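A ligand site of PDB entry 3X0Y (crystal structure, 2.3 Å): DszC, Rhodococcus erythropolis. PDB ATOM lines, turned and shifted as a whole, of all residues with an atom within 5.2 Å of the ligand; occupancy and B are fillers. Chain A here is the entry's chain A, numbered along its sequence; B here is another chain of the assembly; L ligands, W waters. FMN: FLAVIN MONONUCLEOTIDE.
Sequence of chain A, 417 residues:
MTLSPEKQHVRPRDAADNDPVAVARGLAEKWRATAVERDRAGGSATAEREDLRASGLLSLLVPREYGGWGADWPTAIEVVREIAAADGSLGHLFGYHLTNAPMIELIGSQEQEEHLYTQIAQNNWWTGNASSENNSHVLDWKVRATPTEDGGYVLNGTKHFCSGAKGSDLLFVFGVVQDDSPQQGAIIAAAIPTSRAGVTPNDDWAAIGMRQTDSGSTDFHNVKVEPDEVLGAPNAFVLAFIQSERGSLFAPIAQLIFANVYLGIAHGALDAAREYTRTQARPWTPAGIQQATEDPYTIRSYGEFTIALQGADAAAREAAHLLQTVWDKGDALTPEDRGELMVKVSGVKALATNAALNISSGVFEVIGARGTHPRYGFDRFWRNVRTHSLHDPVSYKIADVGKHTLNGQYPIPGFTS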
ATOM      1  N   HIS A  92      16.246  10.737  -0.842  1.00  0.00           N
ATOM      2  CA  HIS A  92      14.821  10.427  -0.807  1.00  0.00           C
ATOM      3  C   HIS A  92      13.992  11.710  -0.770  1.00  0.00           C
ATOM      4  O   HIS A  92      13.042  11.867  -1.535  1.00  0.00           O
ATOM      5  CB  HIS A  92      14.504   9.555   0.405  1.00  0.00           C
ATOM      6  CG  HIS A  92      13.041   9.431   0.713  1.00  0.00           C
ATOM      7  ND1 HIS A  92      12.263   8.397   0.241  1.00  0.00           N
ATOM      8  CD2 HIS A  92      12.220  10.211   1.457  1.00  0.00           C
ATOM      9  CE1 HIS A  92      11.021   8.550   0.670  1.00  0.00           C
ATOM     10  NE2 HIS A  92      10.972   9.639   1.413  1.00  0.00           N
ATOM     11  N   TYR A  96      11.705  12.804  -3.799  1.00  0.00           N
ATOM     12  CA  TYR A  96      10.249  12.950  -3.660  1.00  0.00           C
ATOM     13  C   TYR A  96       9.762  14.344  -4.045  1.00  0.00           C
ATOM     14  O   TYR A  96       8.721  14.479  -4.671  1.00  0.00           O
ATOM     15  CB  TYR A  96       9.763  12.616  -2.242  1.00  0.00           C
ATOM     16  CG  TYR A  96       8.860  11.410  -2.203  1.00  0.00           C
ATOM     17  CD1 TYR A  96       7.522  11.527  -2.586  1.00  0.00           C
ATOM     18  CD2 TYR A  96       9.330  10.166  -1.811  1.00  0.00           C
ATOM     19  CE1 TYR A  96       6.678  10.425  -2.561  1.00  0.00           C
ATOM     20  CE2 TYR A  96       8.486   9.064  -1.786  1.00  0.00           C
ATOM     21  CZ  TYR A  96       7.164   9.196  -2.166  1.00  0.00           C
ATOM     22  OH  TYR A  96       6.329   8.097  -2.142  1.00  0.00           O
ATOM     23  N   ASN A 129       4.237  15.658   0.444  1.00  0.00           N
ATOM     24  CA  ASN A 129       2.989  15.029   0.040  1.00  0.00           C
ATOM     25  C   ASN A 129       2.317  14.327   1.209  1.00  0.00           C
ATOM     26  O   ASN A 129       2.946  14.036   2.232  1.00  0.00           O
ATOM     27  CB  ASN A 129       3.220  14.028  -1.083  1.00  0.00           C
ATOM     28  CG  ASN A 129       3.946  12.787  -0.618  1.00  0.00           C
ATOM     29  OD1 ASN A 129       3.336  11.743  -0.407  1.00  0.00           O
ATOM     30  ND2 ASN A 129       5.252  12.891  -0.426  1.00  0.00           N
ATOM     31  N   SER A 131      -0.431  11.248   1.052  1.00  0.00           N
ATOM     32  CA  SER A 131      -1.158  10.394   0.107  1.00  0.00           C
ATOM     33  C   SER A 131      -1.499   9.010   0.660  1.00  0.00           C
ATOM     34  O   SER A 131      -2.651   8.590   0.569  1.00  0.00           O
ATOM     35  CB  SER A 131      -0.351  10.262  -1.189  1.00  0.00           C
ATOM     36  OG  SER A 131       0.192  11.509  -1.571  1.00  0.00           O
ATOM     37  N   SER A 132      -0.507   8.313   1.210  1.00  0.00           N
ATOM     38  CA  SER A 132      -0.724   6.971   1.755  1.00  0.00           C
ATOM     39  C   SER A 132      -1.302   7.008   3.169  1.00  0.00           C
ATOM     40  O   SER A 132      -1.067   7.942   3.920  1.00  0.00           O
ATOM     41  CB  SER A 132       0.587   6.180   1.764  1.00  0.00           C
ATOM     42  OG  SER A 132       0.969   5.828   0.439  1.00  0.00           O
ATOM     43  N   VAL A 138      -3.430  -0.614   0.868  1.00  0.00           N
ATOM     44  CA  VAL A 138      -2.980   0.657   0.263  1.00  0.00           C
ATOM     45  C   VAL A 138      -3.996   1.362  -0.659  1.00  0.00           C
ATOM     46  O   VAL A 138      -3.917   2.579  -0.836  1.00  0.00           O
ATOM     47  CB  VAL A 138      -1.633   0.485  -0.485  1.00  0.00           C
ATOM     48  CG1 VAL A 138      -0.515   0.178   0.506  1.00  0.00           C
ATOM     49  CG2 VAL A 138      -1.713  -0.589  -1.558  1.00  0.00           C
ATOM     50  N   PHE A 161       2.410   8.233   5.730  1.00  0.00           N
ATOM     51  CA  PHE A 161       3.763   8.262   5.177  1.00  0.00           C
ATOM     52  C   PHE A 161       3.974   9.559   4.419  1.00  0.00           C
ATOM     53  O   PHE A 161       4.071   9.571   3.199  1.00  0.00           O
ATOM     54  CB  PHE A 161       4.005   7.069   4.239  1.00  0.00           C
ATOM     55  CG  PHE A 161       4.220   5.756   4.944  1.00  0.00           C
ATOM     56  CD1 PHE A 161       5.471   5.413   5.441  1.00  0.00           C
ATOM     57  CD2 PHE A 161       3.183   4.836   5.064  1.00  0.00           C
ATOM     58  CE1 PHE A 161       5.672   4.189   6.064  1.00  0.00           C
ATOM     59  CE2 PHE A 161       3.384   3.612   5.686  1.00  0.00           C
ATOM     60  CZ  PHE A 161       4.629   3.287   6.191  1.00  0.00           C
ATOM     61  N   CYS A 162       4.044  10.668   5.148  1.00  0.00           N
ATOM     62  CA  CYS A 162       4.051  11.997   4.538  1.00  0.00           C
ATOM     63  C   CYS A 162       5.456  12.579   4.438  1.00  0.00           C
ATOM     64  O   CYS A 162       5.808  13.508   5.155  1.00  0.00           O
ATOM     65  CB  CYS A 162       3.159  12.937   5.358  1.00  0.00           C
ATOM     66  SG  CYS A 162       1.560  12.231   5.782  1.00  0.00           S
ATOM     67  N   SER A 163       6.258  12.023   3.534  1.00  0.00           N
ATOM     68  CA  SER A 163       7.634  12.484   3.328  1.00  0.00           C
ATOM     69  C   SER A 163       7.668  13.955   2.930  1.00  0.00           C
ATOM     70  O   SER A 163       6.997  14.388   1.992  1.00  0.00           O
ATOM     71  CB  SER A 163       8.326  11.656   2.240  1.00  0.00           C
ATOM     72  OG  SER A 163       8.383  10.280   2.592  1.00  0.00           O
ATOM     73  N   TRP A 205       7.848  10.416  13.048  1.00  0.00           N
ATOM     74  CA  TRP A 205       8.484   9.472  12.133  1.00  0.00           C
ATOM     75  C   TRP A 205       9.625   8.731  12.813  1.00  0.00           C
ATOM     76  O   TRP A 205      10.574   9.349  13.289  1.00  0.00           O
ATOM     77  CB  TRP A 205       9.007  10.195  10.891  1.00  0.00           C
ATOM     78  CG  TRP A 205       9.860   9.330  10.000  1.00  0.00           C
ATOM     79  CD1 TRP A 205      11.165   9.541   9.667  1.00  0.00           C
ATOM     80  CD2 TRP A 205       9.469   8.117   9.333  1.00  0.00           C
ATOM     81  NE1 TRP A 205      11.610   8.548   8.833  1.00  0.00           N
ATOM     82  CE2 TRP A 205      10.596   7.660   8.613  1.00  0.00           C
ATOM     83  CE3 TRP A 205       8.277   7.380   9.290  1.00  0.00           C
ATOM     84  CZ2 TRP A 205      10.565   6.490   7.843  1.00  0.00           C
ATOM     85  CZ3 TRP A 205       8.253   6.222   8.523  1.00  0.00           C
ATOM     86  CH2 TRP A 205       9.384   5.786   7.811  1.00  0.00           C
ATOM     87  N   MET A 210      16.196   5.539   6.724  1.00  0.00           N
ATOM     88  CA  MET A 210      15.550   6.752   6.200  1.00  0.00           C
ATOM     89  C   MET A 210      15.094   7.645   7.356  1.00  0.00           C
ATOM     90  O   MET A 210      14.012   8.250   7.309  1.00  0.00           O
ATOM     91  CB  MET A 210      14.376   6.386   5.276  1.00  0.00           C
ATOM     92  CG  MET A 210      14.791   5.747   3.953  1.00  0.00           C
ATOM     93  SD  MET A 210      15.917   6.769   2.997  1.00  0.00           S
ATOM     94  CE  MET A 210      16.026   5.814   1.480  1.00  0.00           C
ATOM     95  N   THR A 213      13.692  11.432   6.853  1.00  0.00           N
ATOM     96  CA  THR A 213      12.799  11.706   5.709  1.00  0.00           C
ATOM     97  C   THR A 213      11.507  12.386   6.143  1.00  0.00           C
ATOM     98  O   THR A 213      10.741  12.831   5.292  1.00  0.00           O
ATOM     99  CB  THR A 213      12.475  10.426   4.907  1.00  0.00           C
ATOM    100  OG1 THR A 213      11.880   9.439   5.745  1.00  0.00           O
ATOM    101  CG2 THR A 213      13.725   9.869   4.267  1.00  0.00           C
ATOM    102  N   SER A 215       8.758  11.162   7.265  1.00  0.00           N
ATOM    103  CA  SER A 215       7.611  10.456   6.694  1.00  0.00           C
ATOM    104  C   SER A 215       6.597  10.102   7.787  1.00  0.00           C
ATOM    105  O   SER A 215       6.125   8.968   7.862  1.00  0.00           O
ATOM    106  CB  SER A 215       8.092   9.184   5.975  1.00  0.00           C
ATOM    107  OG  SER A 215       9.068   9.481   4.985  1.00  0.00           O
ATOM    108  N   THR A 387      14.970  -0.161   4.463  1.00  0.00           N
ATOM    109  CA  THR A 387      13.759   0.575   4.774  1.00  0.00           C
ATOM    110  C   THR A 387      12.975   0.944   3.516  1.00  0.00           C
ATOM    111  O   THR A 387      11.844   0.508   3.350  1.00  0.00           O
ATOM    112  CB  THR A 387      14.067   1.842   5.596  1.00  0.00           C
ATOM    113  OG1 THR A 387      14.633   1.461   6.856  1.00  0.00           O
ATOM    114  CG2 THR A 387      12.795   2.654   5.848  1.00  0.00           C
ATOM    115  N   HIS A 388      13.557   1.773   2.641  1.00  0.00           N
ATOM    116  CA  HIS A 388      12.784   2.288   1.524  1.00  0.00           C
ATOM    117  C   HIS A 388      12.453   1.243   0.466  1.00  0.00           C
ATOM    118  O   HIS A 388      11.429   1.354  -0.195  1.00  0.00           O
ATOM    119  CB  HIS A 388      13.433   3.489   0.856  1.00  0.00           C
ATOM    120  CG  HIS A 388      12.479   4.236  -0.040  1.00  0.00           C
ATOM    121  ND1 HIS A 388      12.205   3.834  -1.329  1.00  0.00           N
ATOM    122  CD2 HIS A 388      11.705   5.324   0.195  1.00  0.00           C
ATOM    123  CE1 HIS A 388      11.328   4.661  -1.861  1.00  0.00           C
ATOM    124  NE2 HIS A 388      11.009   5.574  -0.962  1.00  0.00           N
ATOM    125  N   LEU A 390      11.041  -1.263   0.827  1.00  0.00           N
ATOM    126  CA  LEU A 390       9.694  -1.724   1.180  1.00  0.00           C
ATOM    127  C   LEU A 390       8.567  -0.748   0.828  1.00  0.00           C
ATOM    128  O   LEU A 390       7.406  -1.016   1.134  1.00  0.00           O
ATOM    129  CB  LEU A 390       9.641  -2.042   2.687  1.00  0.00           C
ATOM    130  CG  LEU A 390      10.704  -3.020   3.203  1.00  0.00           C
ATOM    131  CD1 LEU A 390      10.638  -3.172   4.711  1.00  0.00           C
ATOM    132  CD2 LEU A 390      10.564  -4.386   2.518  1.00  0.00           C
ATOM    133  N   HIS A 391       8.891   0.389   0.206  1.00  0.00           N
ATOM    134  CA  HIS A 391       7.887   1.358  -0.248  1.00  0.00           C
ATOM    135  C   HIS A 391       6.768   0.635  -0.994  1.00  0.00           C
ATOM    136  O   HIS A 391       5.586   0.808  -0.699  1.00  0.00           O
ATOM    137  CB  HIS A 391       8.528   2.418  -1.143  1.00  0.00           C
ATOM    138  CG  HIS A 391       7.579   3.468  -1.641  1.00  0.00           C
ATOM    139  ND1 HIS A 391       6.813   3.298  -2.772  1.00  0.00           N
ATOM    140  CD2 HIS A 391       7.262   4.686  -1.147  1.00  0.00           C
ATOM    141  CE1 HIS A 391       6.072   4.378  -2.960  1.00  0.00           C
ATOM    142  NE2 HIS A 391       6.326   5.230  -1.983  1.00  0.00           N
ATOM    143  N   ASP A 392       7.170  -0.188  -1.961  1.00  0.00           N
ATOM    144  CA  ASP A 392       6.249  -1.086  -2.659  1.00  0.00           C
ATOM    145  C   ASP A 392       6.988  -2.373  -3.007  1.00  0.00           C
ATOM    146  O   ASP A 392       8.223  -2.362  -3.143  1.00  0.00           O
ATOM    147  CB  ASP A 392       5.669  -0.411  -3.901  1.00  0.00           C
ATOM    148  CG  ASP A 392       6.731   0.113  -4.830  1.00  0.00           C
ATOM    149  OD1 ASP A 392       7.140   1.284  -4.672  1.00  0.00           O
ATOM    150  OD2 ASP A 392       7.168  -0.647  -5.735  1.00  0.00           O
ATOM    151  N   TYR B 276       4.263 -11.472  12.410  1.00  0.00           N
ATOM    152  CA  TYR B 276       3.859 -10.215  11.750  1.00  0.00           C
ATOM    153  C   TYR B 276       3.046 -10.458  10.469  1.00  0.00           C
ATOM    154  O   TYR B 276       2.054  -9.774  10.229  1.00  0.00           O
ATOM    155  CB  TYR B 276       5.099  -9.368  11.424  1.00  0.00           C
ATOM    156  CG  TYR B 276       4.778  -7.938  11.022  1.00  0.00           C
ATOM    157  CD1 TYR B 276       4.303  -7.645   9.743  1.00  0.00           C
ATOM    158  CD2 TYR B 276       4.952  -6.891  11.914  1.00  0.00           C
ATOM    159  CE1 TYR B 276       4.011  -6.331   9.367  1.00  0.00           C
ATOM    160  CE2 TYR B 276       4.662  -5.581  11.547  1.00  0.00           C
ATOM    161  CZ  TYR B 276       4.194  -5.309  10.270  1.00  0.00           C
ATOM    162  OH  TYR B 276       3.910  -4.016   9.896  1.00  0.00           O
ATOM    163  N   ARG B 282      -0.296  -6.409   5.281  1.00  0.00           N
ATOM    164  CA  ARG B 282      -1.446  -6.073   4.459  1.00  0.00           C
ATOM    165  C   ARG B 282      -1.267  -6.650   3.062  1.00  0.00           C
ATOM    166  O   ARG B 282      -0.145  -6.740   2.561  1.00  0.00           O
ATOM    167  CB  ARG B 282      -1.617  -4.566   4.374  1.00  0.00           C
ATOM    168  CG  ARG B 282      -1.706  -3.889   5.738  1.00  0.00           C
ATOM    169  CD  ARG B 282      -1.967  -2.400   5.630  1.00  0.00           C
ATOM    170  NE  ARG B 282      -0.947  -1.695   4.855  1.00  0.00           N
ATOM    171  CZ  ARG B 282      -0.902  -0.376   4.680  1.00  0.00           C
ATOM    172  NH1 ARG B 282      -1.810   0.415   5.260  1.00  0.00           N
ATOM    173  NH2 ARG B 282       0.060   0.165   3.950  1.00  0.00           N
ATOM    174  N   ILE B 367       7.521  -8.667   5.595  1.00  0.00           N
ATOM    175  CA  ILE B 367       7.038  -7.860   6.722  1.00  0.00           C
ATOM    176  C   ILE B 367       6.414  -6.547   6.244  1.00  0.00           C
ATOM    177  O   ILE B 367       5.253  -6.282   6.527  1.00  0.00           O
ATOM    178  CB  ILE B 367       8.154  -7.583   7.754  1.00  0.00           C
ATOM    179  CG1 ILE B 367       8.411  -8.846   8.580  1.00  0.00           C
ATOM    180  CG2 ILE B 367       7.763  -6.450   8.697  1.00  0.00           C
ATOM    181  CD1 ILE B 367       9.660  -8.777   9.432  1.00  0.00           C
ATOM    182  N   GLY B 368       7.191  -5.737   5.522  1.00  0.00           N
ATOM    183  CA  GLY B 368       6.676  -4.483   4.946  1.00  0.00           C
ATOM    184  C   GLY B 368       7.146  -3.217   5.651  1.00  0.00           C
ATOM    185  O   GLY B 368       7.762  -3.272   6.723  1.00  0.00           O
ATOM    186  N   ALA B 369       6.817  -2.083   5.039  1.00  0.00           N
ATOM    187  CA  ALA B 369       7.318  -0.763   5.465  1.00  0.00           C
ATOM    188  C   ALA B 369       7.069  -0.408   6.930  1.00  0.00           C
ATOM    189  O   ALA B 369       7.967   0.080   7.616  1.00  0.00           O
ATOM    190  CB  ALA B 369       6.747   0.321   4.563  1.00  0.00           C
ATOM    191  N   ARG B 370       5.852  -0.669   7.413  1.00  0.00           N
ATOM    192  CA  ARG B 370       5.493  -0.314   8.800  1.00  0.00           C
ATOM    193  C   ARG B 370       6.287  -1.131   9.818  1.00  0.00           C
ATOM    194  O   ARG B 370       6.520  -0.665  10.933  1.00  0.00           O
ATOM    195  CB  ARG B 370       3.990  -0.518   9.031  1.00  0.00           C
ATOM    196  CG  ARG B 370       3.099   0.396   8.187  1.00  0.00           C
ATOM    197  CD  ARG B 370       1.649  -0.058   8.247  1.00  0.00           C
ATOM    198  NE  ARG B 370       1.526  -1.480   7.907  1.00  0.00           N
ATOM    199  CZ  ARG B 370       0.592  -2.303   8.393  1.00  0.00           C
ATOM    200  NH1 ARG B 370      -0.339  -1.875   9.240  1.00  0.00           N
ATOM    201  NH2 ARG B 370       0.588  -3.583   8.021  1.00  0.00           N
ATOM    202  N   GLY B 371       6.717  -2.322   9.422  1.00  0.00           N
ATOM    203  CA  GLY B 371       7.562  -3.162  10.270  1.00  0.00           C
ATOM    204  C   GLY B 371       8.959  -2.625  10.524  1.00  0.00           C
ATOM    205  O   GLY B 371       9.689  -3.189  11.336  1.00  0.00           O
HETATM  206  N1  FMN L   1       3.725   6.916   0.709  1.00  0.00           N
HETATM  207  C2  FMN L   1       3.272   8.091   0.201  1.00  0.00           C
HETATM  208  O2  FMN L   1       2.107   8.121  -0.248  1.00  0.00           O
HETATM  209  N3  FMN L   1       4.023   9.212   0.146  1.00  0.00           N
HETATM  210  C4  FMN L   1       5.288   9.231   0.605  1.00  0.00           C
HETATM  211  O4  FMN L   1       5.971  10.278   0.567  1.00  0.00           O
HETATM  212  C4A FMN L   1       5.852   7.990   1.187  1.00  0.00           C
HETATM  213  N5  FMN L   1       7.120   7.941   1.675  1.00  0.00           N
HETATM  214  C5A FMN L   1       7.617   6.796   2.197  1.00  0.00           C
HETATM  215  C6  FMN L   1       8.922   6.793   2.684  1.00  0.00           C
HETATM  216  C7  FMN L   1       9.477   5.635   3.224  1.00  0.00           C
HETATM  217  C7M FMN L   1      10.888   5.638   3.748  1.00  0.00           C
HETATM  218  C8  FMN L   1       8.662   4.389   3.286  1.00  0.00           C
HETATM  219  C8M FMN L   1       9.258   3.145   3.872  1.00  0.00           C
HETATM  220  C9  FMN L   1       7.358   4.389   2.808  1.00  0.00           C
HETATM  221  C9A FMN L   1       6.781   5.547   2.251  1.00  0.00           C
HETATM  222  N10 FMN L   1       5.455   5.573   1.723  1.00  0.00           N
HETATM  223  C10 FMN L   1       4.976   6.791   1.203  1.00  0.00           C
HETATM  224  C1' FMN L   1       4.546   4.419   1.794  1.00  0.00           C
HETATM  225  C2' FMN L   1       4.260   3.559   0.581  1.00  0.00           C
HETATM  226  O2' FMN L   1       3.573   4.343  -0.416  1.00  0.00           O
HETATM  227  C3' FMN L   1       3.356   2.387   1.003  1.00  0.00           C
HETATM  228  O3' FMN L   1       2.066   2.893   1.369  1.00  0.00           O
HETATM  229  C4' FMN L   1       3.869   1.587   2.198  1.00  0.00           C
HETATM  230  O4' FMN L   1       5.276   1.340   2.073  1.00  0.00           O
HETATM  231  C5' FMN L   1       3.143   0.249   2.350  1.00  0.00           C
HETATM  232  O5' FMN L   1       3.132  -0.120   3.743  1.00  0.00           O
HETATM  233  P   FMN L   1       3.146  -1.665   4.190  1.00  0.00           P
HETATM  234  O1P FMN L   1       3.266  -1.618   5.686  1.00  0.00           O
HETATM  235  O2P FMN L   1       1.825  -2.189   3.677  1.00  0.00           O
HETATM  236  O3P FMN L   1       4.366  -2.235   3.507  1.00  0.00           O
HETATM  237  O   HOH W   1       4.355  -3.687   7.147  1.00  0.00           O
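The backbone NH of Ser 132 lies within hydrogen-bond range of an oxygen (O2) of the ligand (3.0 Å).
The side-chain hydroxyl (OG) of Ser 132 lies within hydrogen-bond range of an oxygen (O2) of the ligand (2.7 Å).
The side-chain amide oxygen (OD1) of Asn 129 lies within hydrogen-bond range of a nitrogen (N3) of the ligand (2.7 Å).
The backbone NH (N) of Ser 163 sits close to an oxygen (O4) of the ligand (3.5 Å).
A nitrogen (N5) of the ligand is in hydrogen-bond range of the side-chain hydroxyl (OG) of Ser 163 (2.8 Å).
An oxygen (O1P) of the ligand lies close to the backbone NH of Arg 370 of chain B (3.3 Å).
The guanidinium group (NE) of Arg 370 of chain B is in salt-bridge range of an oxygen (O1P) of the ligand (2.8 Å).
The backbone carbonyl oxygen (O) of His 391 lies within hydrogen-bond range of an oxygen (O4') of the ligand, 2.8 Å away.
NE2 of His 391 sits at hydrogen-bond distance from O2' of the ligand (3.3 Å).
O of Phe 161 lies close to N3 of the ligand, 3.1 Å away.
O3P of the ligand lies within hydrogen-bond range of N of Ala 369 of chain B (2.9 Å).
The guanidinium group (NH2) of Arg 282 of chain B is in salt-bridge range of an oxygen (O2P) of the ligand, 3.0 Å away.
N3 of the ligand sits close to OH of Tyr 96 (3.4 Å).
O4' of the ligand sits at hydrogen-bond distance from O of Leu 390, 3.3 Å away.
The side-chain amide nitrogen (ND2) of Asn 129 sits at hydrogen-bond distance from the backbone carbonyl oxygen (O) of Ser 163 (3.3 Å).
OD1 of Asn 129 lies within hydrogen-bond range of OG of Ser 131 (3.4 Å).
The side-chain hydroxyl of Ser 215 is in hydrogen-bond range of the side-chain hydroxyl of Ser 163.
A ring nitrogen (NE2) of His 391 lies within hydrogen-bond range of the side-chain hydroxyl (OH) of Tyr 96.
A ring nitrogen (ND1) of His 391 sits at hydrogen-bond distance from the side-chain carboxylate (OD1) of Asp 392, at 2.8 Å.
OG1 of Thr 213 sits at hydrogen-bond distance from OG of Ser 215 (2.9 Å).
The indole nitrogen (NE1) of Trp 205 sits at hydrogen-bond distance from the backbone carbonyl oxygen (O) of Met 210 (2.9 Å).
O of Met 210 is in hydrogen-bond range of OG1 of Thr 213, 2.9 Å away.
Merely in contact with the ligand: Ser 131, His 92, Gly 368 of chain B, Ser 215, His 388, Thr 387, Val 138 and Met 210.
Hydrophobic or aromatic side chains that line the ligand: His 92, Tyr 96, Val 138, Phe 161, Met 210, His 388, His 391 and Ala 369 of chain B.
Of the 25 residues printed, 18 come within 4 Å of the ligand.
The nearest printed residue that does not touch the ligand is Trp 205 (4.2 Å).
Water W1 lies within hydrogen-bond range of O1P of the ligand (2.8 Å), OH of Tyr 276 of chain B (2.8 Å), O of Ile 367 of chain B (2.8 Å), N of Arg 370 of chain B (3.4 Å) and O of Gly 368 of chain B (3.5 Å).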
